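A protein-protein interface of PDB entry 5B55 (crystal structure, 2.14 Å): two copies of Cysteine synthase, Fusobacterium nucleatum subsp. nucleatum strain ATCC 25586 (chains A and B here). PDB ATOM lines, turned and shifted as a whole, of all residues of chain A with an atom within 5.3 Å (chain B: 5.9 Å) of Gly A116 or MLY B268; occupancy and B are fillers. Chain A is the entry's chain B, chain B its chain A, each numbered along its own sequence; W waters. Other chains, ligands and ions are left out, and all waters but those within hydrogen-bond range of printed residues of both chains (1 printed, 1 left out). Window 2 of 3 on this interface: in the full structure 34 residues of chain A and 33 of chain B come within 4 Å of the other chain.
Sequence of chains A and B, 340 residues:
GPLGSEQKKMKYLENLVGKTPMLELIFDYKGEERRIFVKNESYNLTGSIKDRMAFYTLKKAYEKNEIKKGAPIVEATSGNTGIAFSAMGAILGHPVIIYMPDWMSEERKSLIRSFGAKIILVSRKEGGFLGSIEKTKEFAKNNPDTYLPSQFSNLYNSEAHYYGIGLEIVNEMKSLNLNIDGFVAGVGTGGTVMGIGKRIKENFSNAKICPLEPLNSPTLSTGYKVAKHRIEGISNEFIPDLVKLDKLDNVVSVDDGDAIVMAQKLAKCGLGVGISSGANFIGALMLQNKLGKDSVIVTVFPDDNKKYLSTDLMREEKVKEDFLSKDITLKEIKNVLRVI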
ATOM      1  N   ALA A  90      11.263 -13.240   1.543  1.00  0.00           N
ATOM      2  CA  ALA A  90      10.007 -13.256   2.279  1.00  0.00           C
ATOM      3  C   ALA A  90       9.824 -14.611   2.981  1.00  0.00           C
ATOM      4  O   ALA A  90       9.428 -14.645   4.122  1.00  0.00           O
ATOM      5  CB  ALA A  90       8.829 -12.990   1.361  1.00  0.00           C
ATOM      6  N   VAL A  96      12.992  -6.931   2.021  1.00  0.00           N
ATOM      7  CA  VAL A  96      13.748  -6.878   0.791  1.00  0.00           C
ATOM      8  C   VAL A  96      13.542  -5.528   0.153  1.00  0.00           C
ATOM      9  O   VAL A  96      12.412  -5.002   0.099  1.00  0.00           O
ATOM     10  CB  VAL A  96      13.353  -8.028  -0.176  1.00  0.00           C
ATOM     11  CG1 VAL A  96      14.153  -7.931  -1.480  1.00  0.00           C
ATOM     12  CG2 VAL A  96      13.560  -9.411   0.490  1.00  0.00           C
ATOM     13  N   ILE A 112       7.696  -7.640  -8.077  1.00  0.00           N
ATOM     14  CA  ILE A 112       8.544  -7.375  -6.902  1.00  0.00           C
ATOM     15  C   ILE A 112       7.706  -6.811  -5.724  1.00  0.00           C
ATOM     16  O   ILE A 112       7.856  -7.216  -4.571  1.00  0.00           O
ATOM     17  CB  ILE A 112       9.700  -6.398  -7.283  1.00  0.00           C
ATOM     18  CG1 ILE A 112      10.686  -7.094  -8.240  1.00  0.00           C
ATOM     19  CG2 ILE A 112      10.426  -5.886  -6.057  1.00  0.00           C
ATOM     20  CD1 ILE A 112      11.583  -6.140  -9.026  1.00  0.00           C
ATOM     21  N   ARG A 113       6.805  -5.910  -6.037  1.00  0.00           N
ATOM     22  CA  ARG A 113       5.892  -5.337  -5.026  1.00  0.00           C
ATOM     23  C   ARG A 113       4.919  -6.437  -4.506  1.00  0.00           C
ATOM     24  O   ARG A 113       4.661  -6.531  -3.330  1.00  0.00           O
ATOM     25  CB  ARG A 113       5.223  -4.077  -5.641  1.00  0.00           C
ATOM     26  CG  ARG A 113       4.061  -3.402  -4.922  1.00  0.00           C
ATOM     27  CD  ARG A 113       3.681  -2.108  -5.678  1.00  0.00           C
ATOM     28  NE  ARG A 113       2.920  -2.367  -6.936  1.00  0.00           N
ATOM     29  CZ  ARG A 113       3.206  -1.909  -8.175  1.00  0.00           C
ATOM     30  NH1 ARG A 113       4.268  -1.137  -8.408  1.00  0.00           N
ATOM     31  NH2 ARG A 113       2.415  -2.234  -9.215  1.00  0.00           N
ATOM     32  N   SER A 114       4.427  -7.305  -5.373  1.00  0.00           N
ATOM     33  CA  SER A 114       3.511  -8.401  -4.939  1.00  0.00           C
ATOM     34  C   SER A 114       4.169  -9.305  -3.897  1.00  0.00           C
ATOM     35  O   SER A 114       3.522  -9.788  -2.970  1.00  0.00           O
ATOM     36  CB  SER A 114       3.039  -9.234  -6.163  1.00  0.00           C
ATOM     37  OG  SER A 114       4.013 -10.187  -6.610  1.00  0.00           O
ATOM     38  N   PHE A 115       5.480  -9.494  -3.990  1.00  0.00           N
ATOM     39  CA  PHE A 115       6.210 -10.282  -3.006  1.00  0.00           C
ATOM     40  C   PHE A 115       6.543  -9.507  -1.720  1.00  0.00           C
ATOM     41  O   PHE A 115       7.250 -10.020  -0.848  1.00  0.00           O
ATOM     42  CB  PHE A 115       7.469 -10.879  -3.660  1.00  0.00           C
ATOM     43  CG  PHE A 115       7.157 -11.958  -4.652  1.00  0.00           C
ATOM     44  CD1 PHE A 115       6.527 -13.147  -4.211  1.00  0.00           C
ATOM     45  CD2 PHE A 115       7.390 -11.795  -5.995  1.00  0.00           C
ATOM     46  CE1 PHE A 115       6.219 -14.135  -5.105  1.00  0.00           C
ATOM     47  CE2 PHE A 115       7.024 -12.760  -6.896  1.00  0.00           C
ATOM     48  CZ  PHE A 115       6.466 -13.939  -6.449  1.00  0.00           C
ATOM     49  N   GLY A 116       6.049  -8.283  -1.600  1.00  0.00           N
ATOM     50  CA  GLY A 116       6.191  -7.509  -0.343  1.00  0.00           C
ATOM     51  C   GLY A 116       7.502  -6.767  -0.223  1.00  0.00           C
ATOM     52  O   GLY A 116       7.802  -6.223   0.793  1.00  0.00           O
ATOM     53  N   ALA A 117       8.283  -6.734  -1.282  1.00  0.00           N
ATOM     54  CA  ALA A 117       9.549  -5.964  -1.299  1.00  0.00           C
ATOM     55  C   ALA A 117       9.248  -4.504  -1.565  1.00  0.00           C
ATOM     56  O   ALA A 117       8.262  -4.184  -2.218  1.00  0.00           O
ATOM     57  CB  ALA A 117      10.497  -6.515  -2.399  1.00  0.00           C
ATOM     58  N   MLY A 118      10.128  -3.636  -1.103  1.00  0.00           N
ATOM     59  CA  MLY A 118      10.151  -2.228  -1.522  1.00  0.00           C
ATOM     60  CB  MLY A 118      10.868  -1.372  -0.480  1.00  0.00           C
ATOM     61  CG  MLY A 118      10.752   0.143  -0.717  1.00  0.00           C
ATOM     62  CD  MLY A 118      11.817   0.956   0.073  1.00  0.00           C
ATOM     63  CE  MLY A 118      11.458   1.121   1.544  1.00  0.00           C
ATOM     64  NZ  MLY A 118      12.606   0.934   2.501  1.00  0.00           N
ATOM     65  C   MLY A 118      10.874  -2.116  -2.870  1.00  0.00           C
ATOM     66  O   MLY A 118      12.001  -2.589  -3.014  1.00  0.00           O
ATOM     67  N   ALA B 263      -4.639 -14.345  -1.351  1.00  0.00           N
ATOM     68  CA  ALA B 263      -3.624 -14.444  -2.418  1.00  0.00           C
ATOM     69  C   ALA B 263      -2.488 -13.401  -2.222  1.00  0.00           C
ATOM     70  O   ALA B 263      -1.315 -13.721  -2.416  1.00  0.00           O
ATOM     71  CB  ALA B 263      -4.269 -14.267  -3.812  1.00  0.00           C
ATOM     72  N   GLN B 264      -2.861 -12.189  -1.803  1.00  0.00           N
ATOM     73  CA  GLN B 264      -1.876 -11.143  -1.536  1.00  0.00           C
ATOM     74  C   GLN B 264      -0.992 -11.560  -0.378  1.00  0.00           C
ATOM     75  O   GLN B 264       0.225 -11.383  -0.435  1.00  0.00           O
ATOM     76  CB  GLN B 264      -2.532  -9.786  -1.235  1.00  0.00           C
ATOM     77  CG  GLN B 264      -3.208  -9.193  -2.462  1.00  0.00           C
ATOM     78  CD  GLN B 264      -4.058  -7.973  -2.139  1.00  0.00           C
ATOM     79  OE1 GLN B 264      -4.439  -7.766  -1.003  1.00  0.00           O
ATOM     80  NE2 GLN B 264      -4.362  -7.170  -3.161  1.00  0.00           N
ATOM     81  N   MLY B 265      -1.594 -12.126   0.652  1.00  0.00           N
ATOM     82  CA  MLY B 265      -0.814 -12.593   1.774  1.00  0.00           C
ATOM     83  CB  MLY B 265      -1.713 -13.047   2.921  1.00  0.00           C
ATOM     84  CG  MLY B 265      -2.439 -11.894   3.646  1.00  0.00           C
ATOM     85  CD  MLY B 265      -3.147 -12.514   4.875  1.00  0.00           C
ATOM     86  CE  MLY B 265      -3.891 -11.494   5.716  1.00  0.00           C
ATOM     87  NZ  MLY B 265      -3.236 -10.642   6.779  1.00  0.00           N
ATOM     88  CH1 MLY B 265      -4.165 -10.465   7.931  1.00  0.00           C
ATOM     89  CH2 MLY B 265      -1.988 -11.261   7.230  1.00  0.00           C
ATOM     90  C   MLY B 265       0.123 -13.712   1.363  1.00  0.00           C
ATOM     91  O   MLY B 265       1.256 -13.777   1.839  1.00  0.00           O
ATOM     92  N   LEU B 266      -0.348 -14.616   0.504  1.00  0.00           N
ATOM     93  CA  LEU B 266       0.510 -15.720   0.125  1.00  0.00           C
ATOM     94  C   LEU B 266       1.714 -15.136  -0.615  1.00  0.00           C
ATOM     95  O   LEU B 266       2.859 -15.593  -0.396  1.00  0.00           O
ATOM     96  CB  LEU B 266      -0.245 -16.768  -0.667  1.00  0.00           C
ATOM     97  CG  LEU B 266      -1.162 -17.671   0.196  1.00  0.00           C
ATOM     98  CD1 LEU B 266      -2.315 -18.199  -0.662  1.00  0.00           C
ATOM     99  CD2 LEU B 266      -0.409 -18.802   0.852  1.00  0.00           C
ATOM    100  N   ALA B 267       1.492 -14.136  -1.445  1.00  0.00           N
ATOM    101  CA  ALA B 267       2.605 -13.561  -2.207  1.00  0.00           C
ATOM    102  C   ALA B 267       3.595 -12.885  -1.307  1.00  0.00           C
ATOM    103  O   ALA B 267       4.792 -13.016  -1.498  1.00  0.00           O
ATOM    104  CB  ALA B 267       2.134 -12.627  -3.289  1.00  0.00           C
ATOM    105  N   MLY B 268       3.121 -12.272  -0.227  1.00  0.00           N
ATOM    106  CA  MLY B 268       4.047 -11.735   0.762  1.00  0.00           C
ATOM    107  CB  MLY B 268       3.348 -10.702   1.661  1.00  0.00           C
ATOM    108  CG  MLY B 268       3.016  -9.394   0.950  1.00  0.00           C
ATOM    109  CD  MLY B 268       1.960  -8.599   1.742  1.00  0.00           C
ATOM    110  CE  MLY B 268       1.907  -7.120   1.374  1.00  0.00           C
ATOM    111  NZ  MLY B 268       1.302  -6.935   0.017  1.00  0.00           N
ATOM    112  C   MLY B 268       4.803 -12.783   1.608  1.00  0.00           C
ATOM    113  O   MLY B 268       5.733 -12.404   2.313  1.00  0.00           O
ATOM    114  N   CYS B 269       4.442 -14.063   1.583  1.00  0.00           N
ATOM    115  CA  CYS B 269       5.352 -15.116   2.098  1.00  0.00           C
ATOM    116  C   CYS B 269       6.039 -15.882   0.935  1.00  0.00           C
ATOM    117  O   CYS B 269       6.421 -17.012   1.091  1.00  0.00           O
ATOM    118  CB  CYS B 269       4.654 -16.074   3.076  1.00  0.00           C
ATOM    119  SG  CYS B 269       5.842 -17.262   3.942  1.00  0.00           S
ATOM    120  N   GLY B 270       6.176 -15.265  -0.230  1.00  0.00           N
ATOM    121  CA  GLY B 270       6.958 -15.842  -1.330  1.00  0.00           C
ATOM    122  C   GLY B 270       6.212 -16.730  -2.303  1.00  0.00           C
ATOM    123  O   GLY B 270       6.836 -17.329  -3.174  1.00  0.00           O
ATOM    124  N   LEU B 271       4.887 -16.841  -2.156  1.00  0.00           N
ATOM    125  CA  LEU B 271       4.074 -17.711  -2.954  1.00  0.00           C
ATOM    126  C   LEU B 271       3.167 -16.866  -3.810  1.00  0.00           C
ATOM    127  O   LEU B 271       2.071 -16.460  -3.378  1.00  0.00           O
ATOM    128  CB  LEU B 271       3.326 -18.708  -2.088  1.00  0.00           C
ATOM    129  CG  LEU B 271       4.235 -19.617  -1.227  1.00  0.00           C
ATOM    130  CD1 LEU B 271       3.421 -20.459  -0.290  1.00  0.00           C
ATOM    131  CD2 LEU B 271       5.117 -20.503  -2.101  1.00  0.00           C
HETATM  132  O   HOH W   1       7.176  -9.766   2.529  1.00  0.00           O
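Among the printed residues, pairs that only touch across the chains: Ala A90 with MLY B268, Ala A90 with Gly B270, Ser A114 with Ala B267, Ser A114 with MLY B268, Phe A115 with Ala B267, Phe A115 with MLY B268, Phe A115 with Gly B270 and Gly A116 with MLY B268.
No position is printed for both chains.
Water W1 lies within hydrogen-bond range of O of MLY B268 and the backbone carbonyl oxygen (O) of Phe A115.
Of chain B, only MLY B268 (3.9 Å) comes within 4 Å of Gly A116. MLY B268 touches just these residues of chain A: Ala A90 (3.3 Å), Ser A114 (3.7 Å), Phe A115 (3.97 Å) and Gly A116 (3.9 Å). Of the printed residues of chain B, Ala A90 touches MLY B268 (3.3 Å) and Gly B270 (3.8 Å). Of the printed residues of chain A, Ala B267 touches Ser A114 and Phe A115. Of the printed residues of chain A, Gly B270 touches Ala A90 and Phe A115. Of the printed residues of chain B, Ser A114 touches Ala B267 and MLY B268. The nearest residue of chain B that does not touch Gly A116 is Ala B267 (4.9 Å). The nearest residue of chain A that does not touch MLY B268 is Arg A113 (4.8 Å). The nearest printed residue of chain B that does not touch Phe A115 is Leu B271 (4.2 Å).
Along chain A the printed residues that touch a printed residue of chain B span positions 90 to 116. Hydrophobic or aromatic side chains of chain B that line the printed part of chain A: Ala B267. Among the printed residues, 8 pairs touch across the chains. Among the printed residues, no Asp or Glu carboxylate lies within 4 Å of a Lys or Arg side-chain nitrogen of the other chain.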
